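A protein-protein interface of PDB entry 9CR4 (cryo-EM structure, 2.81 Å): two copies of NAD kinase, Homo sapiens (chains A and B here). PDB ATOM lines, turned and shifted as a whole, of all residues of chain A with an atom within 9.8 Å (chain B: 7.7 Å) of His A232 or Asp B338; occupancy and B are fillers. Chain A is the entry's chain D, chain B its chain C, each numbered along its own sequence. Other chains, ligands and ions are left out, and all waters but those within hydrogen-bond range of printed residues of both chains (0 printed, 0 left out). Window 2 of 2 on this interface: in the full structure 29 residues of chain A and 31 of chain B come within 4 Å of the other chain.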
ATOM      1  N   ASP A 226     -16.800  -7.020   6.917  1.00  0.00           N
ATOM      2  CA  ASP A 226     -16.404  -7.171   5.524  1.00  0.00           C
ATOM      3  C   ASP A 226     -17.611  -7.486   4.652  1.00  0.00           C
ATOM      4  O   ASP A 226     -18.521  -8.210   5.066  1.00  0.00           O
ATOM      5  CB  ASP A 226     -15.359  -8.276   5.377  1.00  0.00           C
ATOM      6  CG  ASP A 226     -14.029  -7.909   6.005  1.00  0.00           C
ATOM      7  OD1 ASP A 226     -13.890  -6.760   6.470  1.00  0.00           O
ATOM      8  OD2 ASP A 226     -13.124  -8.768   6.028  1.00  0.00           O
ATOM      9  N   VAL A 227     -17.608  -6.938   3.441  1.00  0.00           N
ATOM     10  CA  VAL A 227     -18.677  -7.142   2.472  1.00  0.00           C
ATOM     11  C   VAL A 227     -18.082  -7.843   1.261  1.00  0.00           C
ATOM     12  O   VAL A 227     -17.205  -7.290   0.587  1.00  0.00           O
ATOM     13  CB  VAL A 227     -19.339  -5.818   2.063  1.00  0.00           C
ATOM     14  CG1 VAL A 227     -20.385  -6.059   0.996  1.00  0.00           C
ATOM     15  CG2 VAL A 227     -19.951  -5.135   3.272  1.00  0.00           C
ATOM     16  N   TYR A 228     -18.557  -9.052   0.983  1.00  0.00           N
ATOM     17  CA  TYR A 228     -18.119  -9.821  -0.170  1.00  0.00           C
ATOM     18  C   TYR A 228     -19.233  -9.874  -1.204  1.00  0.00           C
ATOM     19  O   TYR A 228     -20.390 -10.148  -0.873  1.00  0.00           O
ATOM     20  CB  TYR A 228     -17.707 -11.241   0.228  1.00  0.00           C
ATOM     21  CG  TYR A 228     -16.493 -11.296   1.126  1.00  0.00           C
ATOM     22  CD1 TYR A 228     -16.619 -11.198   2.503  1.00  0.00           C
ATOM     23  CD2 TYR A 228     -15.222 -11.443   0.594  1.00  0.00           C
ATOM     24  CE1 TYR A 228     -15.513 -11.247   3.325  1.00  0.00           C
ATOM     25  CE2 TYR A 228     -14.109 -11.493   1.409  1.00  0.00           C
ATOM     26  CZ  TYR A 228     -14.260 -11.394   2.773  1.00  0.00           C
ATOM     27  OH  TYR A 228     -13.155 -11.443   3.589  1.00  0.00           O
ATOM     28  N   LEU A 229     -18.876  -9.607  -2.457  1.00  0.00           N
ATOM     29  CA  LEU A 229     -19.824  -9.574  -3.563  1.00  0.00           C
ATOM     30  C   LEU A 229     -19.306 -10.506  -4.650  1.00  0.00           C
ATOM     31  O   LEU A 229     -18.282 -10.220  -5.278  1.00  0.00           O
ATOM     32  CB  LEU A 229     -20.000  -8.145  -4.080  1.00  0.00           C
ATOM     33  CG  LEU A 229     -21.074  -7.818  -5.116  1.00  0.00           C
ATOM     34  CD1 LEU A 229     -21.523  -6.381  -4.965  1.00  0.00           C
ATOM     35  CD2 LEU A 229     -20.533  -8.030  -6.502  1.00  0.00           C
ATOM     36  N   ASP A 230     -20.015 -11.614  -4.867  1.00  0.00           N
ATOM     37  CA  ASP A 230     -19.605 -12.648  -5.820  1.00  0.00           C
ATOM     38  C   ASP A 230     -18.209 -13.178  -5.505  1.00  0.00           C
ATOM     39  O   ASP A 230     -17.398 -13.418  -6.401  1.00  0.00           O
ATOM     40  CB  ASP A 230     -19.685 -12.139  -7.260  1.00  0.00           C
ATOM     41  CG  ASP A 230     -21.104 -12.111  -7.788  1.00  0.00           C
ATOM     42  OD1 ASP A 230     -22.037 -12.353  -6.994  1.00  0.00           O
ATOM     43  OD2 ASP A 230     -21.287 -11.847  -8.994  1.00  0.00           O
ATOM     44  N   GLY A 231     -17.925 -13.361  -4.218  1.00  0.00           N
ATOM     45  CA  GLY A 231     -16.679 -13.952  -3.782  1.00  0.00           C
ATOM     46  C   GLY A 231     -15.504 -13.005  -3.686  1.00  0.00           C
ATOM     47  O   GLY A 231     -14.417 -13.438  -3.283  1.00  0.00           O
ATOM     48  N   HIS A 232     -15.676 -11.735  -4.033  1.00  0.00           N
ATOM     49  CA  HIS A 232     -14.599 -10.757  -3.996  1.00  0.00           C
ATOM     50  C   HIS A 232     -14.901  -9.705  -2.940  1.00  0.00           C
ATOM     51  O   HIS A 232     -16.013  -9.171  -2.890  1.00  0.00           O
ATOM     52  CB  HIS A 232     -14.412 -10.096  -5.362  1.00  0.00           C
ATOM     53  CG  HIS A 232     -14.118 -11.065  -6.464  1.00  0.00           C
ATOM     54  ND1 HIS A 232     -14.266 -10.745  -7.797  1.00  0.00           N
ATOM     55  CD2 HIS A 232     -13.675 -12.344  -6.432  1.00  0.00           C
ATOM     56  CE1 HIS A 232     -13.932 -11.787  -8.537  1.00  0.00           C
ATOM     57  NE2 HIS A 232     -13.569 -12.769  -7.734  1.00  0.00           N
ATOM     58  N   LEU A 233     -13.909  -9.408  -2.104  1.00  0.00           N
ATOM     59  CA  LEU A 233     -14.067  -8.396  -1.067  1.00  0.00           C
ATOM     60  C   LEU A 233     -14.106  -7.022  -1.718  1.00  0.00           C
ATOM     61  O   LEU A 233     -13.062  -6.451  -2.048  1.00  0.00           O
ATOM     62  CB  LEU A 233     -12.927  -8.492  -0.060  1.00  0.00           C
ATOM     63  CG  LEU A 233     -12.873  -7.431   1.039  1.00  0.00           C
ATOM     64  CD1 LEU A 233     -14.119  -7.493   1.908  1.00  0.00           C
ATOM     65  CD2 LEU A 233     -11.621  -7.600   1.882  1.00  0.00           C
ATOM     66  N   ILE A 234     -15.311  -6.489  -1.915  1.00  0.00           N
ATOM     67  CA  ILE A 234     -15.443  -5.189  -2.561  1.00  0.00           C
ATOM     68  C   ILE A 234     -14.995  -4.073  -1.627  1.00  0.00           C
ATOM     69  O   ILE A 234     -14.273  -3.157  -2.034  1.00  0.00           O
ATOM     70  CB  ILE A 234     -16.885  -4.973  -3.053  1.00  0.00           C
ATOM     71  CG1 ILE A 234     -17.892  -5.307  -1.953  1.00  0.00           C
ATOM     72  CG2 ILE A 234     -17.153  -5.821  -4.283  1.00  0.00           C
ATOM     73  CD1 ILE A 234     -19.326  -5.059  -2.352  1.00  0.00           C
ATOM     74  N   THR A 235     -15.411  -4.131  -0.364  1.00  0.00           N
ATOM     75  CA  THR A 235     -15.111  -3.058   0.572  1.00  0.00           C
ATOM     76  C   THR A 235     -15.237  -3.577   1.995  1.00  0.00           C
ATOM     77  O   THR A 235     -15.896  -4.585   2.255  1.00  0.00           O
ATOM     78  CB  THR A 235     -16.038  -1.854   0.362  1.00  0.00           C
ATOM     79  OG1 THR A 235     -15.603  -0.765   1.186  1.00  0.00           O
ATOM     80  CG2 THR A 235     -17.472  -2.213   0.719  1.00  0.00           C
ATOM     81  N   THR A 236     -14.580  -2.870   2.909  1.00  0.00           N
ATOM     82  CA  THR A 236     -14.721  -3.083   4.345  1.00  0.00           C
ATOM     83  C   THR A 236     -15.269  -1.794   4.940  1.00  0.00           C
ATOM     84  O   THR A 236     -14.566  -0.778   4.986  1.00  0.00           O
ATOM     85  CB  THR A 236     -13.388  -3.462   4.986  1.00  0.00           C
ATOM     86  OG1 THR A 236     -12.948  -4.724   4.468  1.00  0.00           O
ATOM     87  CG2 THR A 236     -13.532  -3.556   6.498  1.00  0.00           C
ATOM     88  N   ILE A 271     -26.448  -0.699  -1.585  1.00  0.00           N
ATOM     89  CA  ILE A 271     -25.594  -0.797  -0.406  1.00  0.00           C
ATOM     90  C   ILE A 271     -25.339   0.613   0.103  1.00  0.00           C
ATOM     91  O   ILE A 271     -24.744   1.433  -0.606  1.00  0.00           O
ATOM     92  CB  ILE A 271     -24.269  -1.515  -0.703  1.00  0.00           C
ATOM     93  CG1 ILE A 271     -24.532  -2.960  -1.127  1.00  0.00           C
ATOM     94  CG2 ILE A 271     -23.368  -1.483   0.512  1.00  0.00           C
ATOM     95  CD1 ILE A 271     -23.281  -3.735  -1.441  1.00  0.00           C
ATOM     96  N   ILE A 284     -23.644   2.691  -3.166  1.00  0.00           N
ATOM     97  CA  ILE A 284     -23.561   2.055  -4.471  1.00  0.00           C
ATOM     98  C   ILE A 284     -24.779   1.167  -4.648  1.00  0.00           C
ATOM     99  O   ILE A 284     -25.391   0.716  -3.676  1.00  0.00           O
ATOM    100  CB  ILE A 284     -22.269   1.229  -4.641  1.00  0.00           C
ATOM    101  CG1 ILE A 284     -22.229   0.091  -3.626  1.00  0.00           C
ATOM    102  CG2 ILE A 284     -21.050   2.112  -4.477  1.00  0.00           C
ATOM    103  CD1 ILE A 284     -21.105  -0.886  -3.855  1.00  0.00           C
ATOM    104  N   VAL A 290     -27.084 -10.548  -8.155  1.00  0.00           N
ATOM    105  CA  VAL A 290     -25.779 -10.722  -7.541  1.00  0.00           C
ATOM    106  C   VAL A 290     -25.952 -11.441  -6.208  1.00  0.00           C
ATOM    107  O   VAL A 290     -27.017 -11.409  -5.587  1.00  0.00           O
ATOM    108  CB  VAL A 290     -25.067  -9.366  -7.357  1.00  0.00           C
ATOM    109  CG1 VAL A 290     -25.750  -8.545  -6.277  1.00  0.00           C
ATOM    110  CG2 VAL A 290     -23.603  -9.562  -7.063  1.00  0.00           C
ATOM    111  N   GLU A 291     -24.890 -12.110  -5.766  1.00  0.00           N
ATOM    112  CA  GLU A 291     -24.871 -12.818  -4.494  1.00  0.00           C
ATOM    113  C   GLU A 291     -23.963 -12.069  -3.526  1.00  0.00           C
ATOM    114  O   GLU A 291     -22.736 -12.135  -3.645  1.00  0.00           O
ATOM    115  CB  GLU A 291     -24.389 -14.256  -4.684  1.00  0.00           C
ATOM    116  CG  GLU A 291     -24.971 -15.252  -3.696  1.00  0.00           C
ATOM    117  CD  GLU A 291     -24.400 -15.097  -2.302  1.00  0.00           C
ATOM    118  OE1 GLU A 291     -23.215 -14.725  -2.180  1.00  0.00           O
ATOM    119  OE2 GLU A 291     -25.138 -15.348  -1.326  1.00  0.00           O
ATOM    120  N   LEU A 292     -24.566 -11.360  -2.578  1.00  0.00           N
ATOM    121  CA  LEU A 292     -23.837 -10.648  -1.541  1.00  0.00           C
ATOM    122  C   LEU A 292     -23.538 -11.570  -0.367  1.00  0.00           C
ATOM    123  O   LEU A 292     -24.191 -12.597  -0.169  1.00  0.00           O
ATOM    124  CB  LEU A 292     -24.626  -9.431  -1.054  1.00  0.00           C
ATOM    125  CG  LEU A 292     -24.672  -8.212  -1.967  1.00  0.00           C
ATOM    126  CD1 LEU A 292     -25.669  -7.204  -1.437  1.00  0.00           C
ATOM    127  CD2 LEU A 292     -23.297  -7.590  -2.060  1.00  0.00           C
ATOM    128  N   LYS A 293     -22.536 -11.184   0.417  1.00  0.00           N
ATOM    129  CA  LYS A 293     -22.139 -11.955   1.590  1.00  0.00           C
ATOM    130  C   LYS A 293     -21.406 -11.026   2.544  1.00  0.00           C
ATOM    131  O   LYS A 293     -20.317 -10.543   2.226  1.00  0.00           O
ATOM    132  CB  LYS A 293     -21.256 -13.136   1.195  1.00  0.00           C
ATOM    133  CG  LYS A 293     -20.942 -14.088   2.327  1.00  0.00           C
ATOM    134  CD  LYS A 293     -20.165 -15.288   1.819  1.00  0.00           C
ATOM    135  CE  LYS A 293     -19.887 -16.281   2.933  1.00  0.00           C
ATOM    136  NZ  LYS A 293     -19.102 -15.667   4.039  1.00  0.00           N
ATOM    137  N   ILE A 294     -22.002 -10.779   3.707  1.00  0.00           N
ATOM    138  CA  ILE A 294     -21.465  -9.860   4.701  1.00  0.00           C
ATOM    139  C   ILE A 294     -21.063 -10.665   5.928  1.00  0.00           C
ATOM    140  O   ILE A 294     -21.871 -11.432   6.464  1.00  0.00           O
ATOM    141  CB  ILE A 294     -22.487  -8.770   5.070  1.00  0.00           C
ATOM    142  CG1 ILE A 294     -22.746  -7.852   3.880  1.00  0.00           C
ATOM    143  CG2 ILE A 294     -22.005  -7.965   6.253  1.00  0.00           C
ATOM    144  CD1 ILE A 294     -23.702  -6.732   4.185  1.00  0.00           C
ATOM    145  N   MET A 295     -19.819 -10.492   6.369  1.00  0.00           N
ATOM    146  CA  MET A 295     -19.311 -11.214   7.524  1.00  0.00           C
ATOM    147  C   MET A 295     -18.300 -10.343   8.252  1.00  0.00           C
ATOM    148  O   MET A 295     -17.692  -9.448   7.660  1.00  0.00           O
ATOM    149  CB  MET A 295     -18.671 -12.546   7.118  1.00  0.00           C
ATOM    150  CG  MET A 295     -17.532 -12.406   6.121  1.00  0.00           C
ATOM    151  SD  MET A 295     -16.915 -13.996   5.539  1.00  0.00           S
ATOM    152  CE  MET A 295     -16.464 -14.770   7.089  1.00  0.00           C
ATOM    153  N   PRO B 140      -9.903  -0.529 -18.715  1.00  0.00           N
ATOM    154  CA  PRO B 140      -9.413  -1.577 -17.811  1.00  0.00           C
ATOM    155  C   PRO B 140      -8.041  -2.125 -18.178  1.00  0.00           C
ATOM    156  O   PRO B 140      -7.280  -2.532 -17.294  1.00  0.00           O
ATOM    157  CB  PRO B 140     -10.488  -2.662 -17.937  1.00  0.00           C
ATOM    158  CG  PRO B 140     -11.000  -2.498 -19.323  1.00  0.00           C
ATOM    159  CD  PRO B 140     -10.955  -1.023 -19.618  1.00  0.00           C
ATOM    160  N   ALA B 159     -14.759 -11.030 -21.833  1.00  0.00           N
ATOM    161  CA  ALA B 159     -15.972 -10.570 -21.176  1.00  0.00           C
ATOM    162  C   ALA B 159     -16.224  -9.109 -21.522  1.00  0.00           C
ATOM    163  O   ALA B 159     -15.285  -8.314 -21.623  1.00  0.00           O
ATOM    164  CB  ALA B 159     -15.873 -10.740 -19.660  1.00  0.00           C
ATOM    165  N   VAL B 160     -17.499  -8.761 -21.701  1.00  0.00           N
ATOM    166  CA  VAL B 160     -17.884  -7.422 -22.119  1.00  0.00           C
ATOM    167  C   VAL B 160     -18.966  -6.886 -21.191  1.00  0.00           C
ATOM    168  O   VAL B 160     -19.686  -7.639 -20.533  1.00  0.00           O
ATOM    169  CB  VAL B 160     -18.378  -7.389 -23.580  1.00  0.00           C
ATOM    170  CG1 VAL B 160     -17.220  -7.614 -24.538  1.00  0.00           C
ATOM    171  CG2 VAL B 160     -19.462  -8.428 -23.794  1.00  0.00           C
ATOM    172  N   VAL B 161     -19.063  -5.561 -21.147  1.00  0.00           N
ATOM    173  CA  VAL B 161     -20.134  -4.856 -20.452  1.00  0.00           C
ATOM    174  C   VAL B 161     -20.879  -4.025 -21.484  1.00  0.00           C
ATOM    175  O   VAL B 161     -20.290  -3.144 -22.122  1.00  0.00           O
ATOM    176  CB  VAL B 161     -19.599  -3.965 -19.321  1.00  0.00           C
ATOM    177  CG1 VAL B 161     -20.727  -3.148 -18.718  1.00  0.00           C
ATOM    178  CG2 VAL B 161     -18.934  -4.807 -18.259  1.00  0.00           C
ATOM    179  N   HIS B 263     -23.625   0.494 -10.826  1.00  0.00           N
ATOM    180  CA  HIS B 263     -22.894  -0.462 -11.643  1.00  0.00           C
ATOM    181  C   HIS B 263     -23.463  -0.471 -13.059  1.00  0.00           C
ATOM    182  O   HIS B 263     -24.684  -0.392 -13.238  1.00  0.00           O
ATOM    183  CB  HIS B 263     -22.975  -1.858 -11.027  1.00  0.00           C
ATOM    184  CG  HIS B 263     -22.094  -2.867 -11.696  1.00  0.00           C
ATOM    185  ND1 HIS B 263     -22.471  -3.544 -12.835  1.00  0.00           N
ATOM    186  CD2 HIS B 263     -20.858  -3.317 -11.382  1.00  0.00           C
ATOM    187  CE1 HIS B 263     -21.503  -4.366 -13.196  1.00  0.00           C
ATOM    188  NE2 HIS B 263     -20.512  -4.247 -12.332  1.00  0.00           N
ATOM    189  N   ASN B 265     -24.285  -2.580 -15.118  1.00  0.00           N
ATOM    190  CA  ASN B 265     -25.224  -3.629 -15.494  1.00  0.00           C
ATOM    191  C   ASN B 265     -26.624  -3.395 -14.943  1.00  0.00           C
ATOM    192  O   ASN B 265     -27.482  -4.272 -15.083  1.00  0.00           O
ATOM    193  CB  ASN B 265     -24.711  -4.996 -15.034  1.00  0.00           C
ATOM    194  CG  ASN B 265     -23.629  -5.547 -15.937  1.00  0.00           C
ATOM    195  OD1 ASN B 265     -23.573  -5.226 -17.123  1.00  0.00           O
ATOM    196  ND2 ASN B 265     -22.760  -6.381 -15.380  1.00  0.00           N
ATOM    197  N   ILE B 334     -14.803  -4.170 -23.340  1.00  0.00           N
ATOM    198  CA  ILE B 334     -14.196  -5.411 -22.876  1.00  0.00           C
ATOM    199  C   ILE B 334     -13.504  -5.172 -21.542  1.00  0.00           C
ATOM    200  O   ILE B 334     -12.814  -4.163 -21.355  1.00  0.00           O
ATOM    201  CB  ILE B 334     -13.211  -5.947 -23.929  1.00  0.00           C
ATOM    202  CG1 ILE B 334     -13.934  -6.197 -25.252  1.00  0.00           C
ATOM    203  CG2 ILE B 334     -12.547  -7.221 -23.445  1.00  0.00           C
ATOM    204  CD1 ILE B 334     -13.026  -6.667 -26.360  1.00  0.00           C
ATOM    205  N   CYS B 335     -13.687  -6.100 -20.607  1.00  0.00           N
ATOM    206  CA  CYS B 335     -13.043  -6.034 -19.305  1.00  0.00           C
ATOM    207  C   CYS B 335     -11.923  -7.063 -19.202  1.00  0.00           C
ATOM    208  O   CYS B 335     -11.952  -8.119 -19.837  1.00  0.00           O
ATOM    209  CB  CYS B 335     -14.058  -6.255 -18.182  1.00  0.00           C
ATOM    210  SG  CYS B 335     -15.442  -5.100 -18.206  1.00  0.00           S
ATOM    211  N   VAL B 336     -10.927  -6.734 -18.383  1.00  0.00           N
ATOM    212  CA  VAL B 336      -9.744  -7.577 -18.245  1.00  0.00           C
ATOM    213  C   VAL B 336     -10.041  -8.856 -17.471  1.00  0.00           C
ATOM    214  O   VAL B 336      -9.596  -9.937 -17.861  1.00  0.00           O
ATOM    215  CB  VAL B 336      -8.598  -6.771 -17.602  1.00  0.00           C
ATOM    216  CG1 VAL B 336      -8.183  -5.650 -18.522  1.00  0.00           C
ATOM    217  CG2 VAL B 336      -9.026  -6.187 -16.269  1.00  0.00           C
ATOM    218  N   ARG B 337     -10.791  -8.771 -16.372  1.00  0.00           N
ATOM    219  CA  ARG B 337     -11.090  -9.945 -15.559  1.00  0.00           C
ATOM    220  C   ARG B 337     -12.572 -10.291 -15.573  1.00  0.00           C
ATOM    221  O   ARG B 337     -12.932 -11.410 -15.949  1.00  0.00           O
ATOM    222  CB  ARG B 337     -10.597  -9.729 -14.121  1.00  0.00           C
ATOM    223  CG  ARG B 337      -9.324  -8.912 -14.024  1.00  0.00           C
ATOM    224  CD  ARG B 337      -8.756  -8.920 -12.617  1.00  0.00           C
ATOM    225  NE  ARG B 337      -9.659  -8.305 -11.652  1.00  0.00           N
ATOM    226  CZ  ARG B 337      -9.592  -7.037 -11.272  1.00  0.00           C
ATOM    227  NH1 ARG B 337      -8.679  -6.215 -11.762  1.00  0.00           N
ATOM    228  NH2 ARG B 337     -10.462  -6.582 -10.375  1.00  0.00           N
ATOM    229  N   ASP B 338     -13.442  -9.365 -15.187  1.00  0.00           N
ATOM    230  CA  ASP B 338     -14.871  -9.628 -15.117  1.00  0.00           C
ATOM    231  C   ASP B 338     -15.604  -8.296 -15.071  1.00  0.00           C
ATOM    232  O   ASP B 338     -14.999  -7.263 -14.761  1.00  0.00           O
ATOM    233  CB  ASP B 338     -15.219 -10.497 -13.893  1.00  0.00           C
ATOM    234  CG  ASP B 338     -14.822  -9.853 -12.578  1.00  0.00           C
ATOM    235  OD1 ASP B 338     -14.214  -8.764 -12.596  1.00  0.00           O
ATOM    236  OD2 ASP B 338     -15.120 -10.443 -11.518  1.00  0.00           O
ATOM    237  N   PRO B 339     -16.898  -8.280 -15.397  1.00  0.00           N
ATOM    238  CA  PRO B 339     -17.644  -7.014 -15.339  1.00  0.00           C
ATOM    239  C   PRO B 339     -17.701  -6.400 -13.953  1.00  0.00           C
ATOM    240  O   PRO B 339     -17.869  -5.180 -13.833  1.00  0.00           O
ATOM    241  CB  PRO B 339     -19.043  -7.408 -15.836  1.00  0.00           C
ATOM    242  CG  PRO B 339     -19.088  -8.900 -15.766  1.00  0.00           C
ATOM    243  CD  PRO B 339     -17.693  -9.348 -16.021  1.00  0.00           C
ATOM    244  N   VAL B 340     -17.566  -7.203 -12.900  1.00  0.00           N
ATOM    245  CA  VAL B 340     -17.815  -6.730 -11.544  1.00  0.00           C
ATOM    246  C   VAL B 340     -16.545  -6.211 -10.885  1.00  0.00           C
ATOM    247  O   VAL B 340     -16.449  -5.024 -10.550  1.00  0.00           O
ATOM    248  CB  VAL B 340     -18.445  -7.843 -10.691  1.00  0.00           C
ATOM    249  CG1 VAL B 340     -18.559  -7.384  -9.261  1.00  0.00           C
ATOM    250  CG2 VAL B 340     -19.807  -8.220 -11.242  1.00  0.00           C
ATOM    251  N   SER B 341     -15.560  -7.093 -10.687  1.00  0.00           N
ATOM    252  CA  SER B 341     -14.364  -6.711  -9.945  1.00  0.00           C
ATOM    253  C   SER B 341     -13.562  -5.634 -10.660  1.00  0.00           C
ATOM    254  O   SER B 341     -12.811  -4.901 -10.008  1.00  0.00           O
ATOM    255  CB  SER B 341     -13.484  -7.935  -9.686  1.00  0.00           C
ATOM    256  OG  SER B 341     -12.756  -8.295 -10.848  1.00  0.00           O
ATOM    257  N   ASP B 342     -13.699  -5.526 -11.982  1.00  0.00           N
ATOM    258  CA  ASP B 342     -13.065  -4.426 -12.701  1.00  0.00           C
ATOM    259  C   ASP B 342     -13.644  -3.086 -12.268  1.00  0.00           C
ATOM    260  O   ASP B 342     -12.909  -2.105 -12.108  1.00  0.00           O
ATOM    261  CB  ASP B 342     -13.230  -4.623 -14.206  1.00  0.00           C
ATOM    262  CG  ASP B 342     -12.570  -3.526 -15.016  1.00  0.00           C
ATOM    263  OD1 ASP B 342     -11.607  -2.906 -14.519  1.00  0.00           O
ATOM    264  OD2 ASP B 342     -13.026  -3.277 -16.152  1.00  0.00           O
ATOM    265  N   TRP B 343     -14.964  -3.024 -12.079  1.00  0.00           N
ATOM    266  CA  TRP B 343     -15.598  -1.772 -11.681  1.00  0.00           C
ATOM    267  C   TRP B 343     -15.204  -1.367 -10.268  1.00  0.00           C
ATOM    268  O   TRP B 343     -14.937  -0.187 -10.008  1.00  0.00           O
ATOM    269  CB  TRP B 343     -17.116  -1.892 -11.803  1.00  0.00           C
ATOM    270  CG  TRP B 343     -17.833  -0.622 -11.492  1.00  0.00           C
ATOM    271  CD1 TRP B 343     -17.836   0.516 -12.237  1.00  0.00           C
ATOM    272  CD2 TRP B 343     -18.679  -0.368 -10.367  1.00  0.00           C
ATOM    273  NE1 TRP B 343     -18.616   1.472 -11.637  1.00  0.00           N
ATOM    274  CE2 TRP B 343     -19.147   0.951 -10.488  1.00  0.00           C
ATOM    275  CE3 TRP B 343     -19.080  -1.128  -9.266  1.00  0.00           C
ATOM    276  CZ2 TRP B 343     -19.995   1.529  -9.550  1.00  0.00           C
ATOM    277  CZ3 TRP B 343     -19.923  -0.553  -8.337  1.00  0.00           C
ATOM    278  CH2 TRP B 343     -20.371   0.762  -8.485  1.00  0.00           C
ATOM    279  N   PHE B 344     -15.164  -2.323  -9.340  1.00  0.00           N
ATOM    280  CA  PHE B 344     -14.810  -1.994  -7.964  1.00  0.00           C
ATOM    281  C   PHE B 344     -13.346  -1.589  -7.854  1.00  0.00           C
ATOM    282  O   PHE B 344     -13.000  -0.700  -7.069  1.00  0.00           O
ATOM    283  CB  PHE B 344     -15.125  -3.172  -7.047  1.00  0.00           C
ATOM    284  CG  PHE B 344     -16.592  -3.352  -6.785  1.00  0.00           C
ATOM    285  CD1 PHE B 344     -17.235  -2.589  -5.827  1.00  0.00           C
ATOM    286  CD2 PHE B 344     -17.331  -4.271  -7.508  1.00  0.00           C
ATOM    287  CE1 PHE B 344     -18.584  -2.746  -5.588  1.00  0.00           C
ATOM    288  CE2 PHE B 344     -18.682  -4.432  -7.272  1.00  0.00           C
ATOM    289  CZ  PHE B 344     -19.308  -3.668  -6.312  1.00  0.00           C
ATOM    290  N   GLU B 345     -12.471  -2.233  -8.630  1.00  0.00           N
ATOM    291  CA  GLU B 345     -11.074  -1.815  -8.667  1.00  0.00           C
ATOM    292  C   GLU B 345     -10.942  -0.408  -9.230  1.00  0.00           C
ATOM    293  O   GLU B 345     -10.096   0.374  -8.780  1.00  0.00           O
ATOM    294  CB  GLU B 345     -10.252  -2.803  -9.493  1.00  0.00           C
ATOM    295  CG  GLU B 345      -8.795  -2.409  -9.660  1.00  0.00           C
ATOM    296  CD  GLU B 345      -8.117  -3.148 -10.796  1.00  0.00           C
ATOM    297  OE1 GLU B 345      -8.828  -3.783 -11.602  1.00  0.00           O
ATOM    298  OE2 GLU B 345      -6.872  -3.093 -10.882  1.00  0.00           O
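O of Ile A284 sits at hydrogen-bond distance from N of Ile A271, at 2.7 Å. The backbone NH (N) of Ile A234 is in hydrogen-bond range of the backbone carbonyl oxygen (O) of Val A227 (3.2 Å). The backbone NH of Ser B341 is in hydrogen-bond range of the side-chain carboxylate of Asp B338. The side-chain carboxylate of Asp B338 is in hydrogen-bond range of the backbone NH of Asp B342, 3.3 Å away. The side-chain hydroxyl of Ser B341 lies within hydrogen-bond range of the guanidinium group of Arg B337 (2.9 Å).
CD2 of Leu A229 touches CG1 of Val B340, at 3.5 Å. Phe B344 touches Leu A229 (CZ to CD1, 3.8 Å). CE1 of His A232 touches OD2 of Asp B338 (3.5 Å). Ser B341 touches His A232. Ile A234 touches Phe B344 (CG2 to CG, 3.6 Å). CD1 of Ile A284 touches CE1 of Phe B344, at 3.6 Å.
No position is printed for both chains.
His A232 touches just these residues of chain B: Asp B338 (3.5 Å) and Ser B341 (3.5 Å). Asp B338 touches just one residue of chain A: His A232 (3.5 Å). No residue of chain A comes within 4 Å of Pro B339. Of chain A, only Leu A229 (3.5 Å) comes within 4 Å of Val B340. Of the printed residues of chain B, Ile A284 touches Phe B344. Printed residues of chain B within 4 Å of Leu A229: Val B340 (3.5 Å) and Phe B344 (3.8 Å). Of the printed residues of chain A, Phe B344 touches Leu A229, Ile A234 and Ile A284. Of the printed residues of chain B, Ile A234 touches Phe B344.
Of the 18 printed residues of chain B, 4 touch a printed residue of chain A. Printed residues of chain B that touch a printed residue of chain A: Asp B338, Val B340, Ser B341 and Phe B344. Hydrophobic or aromatic side chains of chain B within 4 Å of the printed part of chain A: Val B340 and Phe B344. Of the 19 printed residues of chain A, 4 touch a printed residue of chain B. Printed residues of chain A that touch a printed residue of chain B: Leu A229, His A232, Ile A234 and Ile A284. Among the printed residues, 6 pairs touch across the chains. Among the printed residues, no Asp or Glu carboxylate lies within 4 Å of a Lys or Arg side-chain nitrogen of the other chain.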
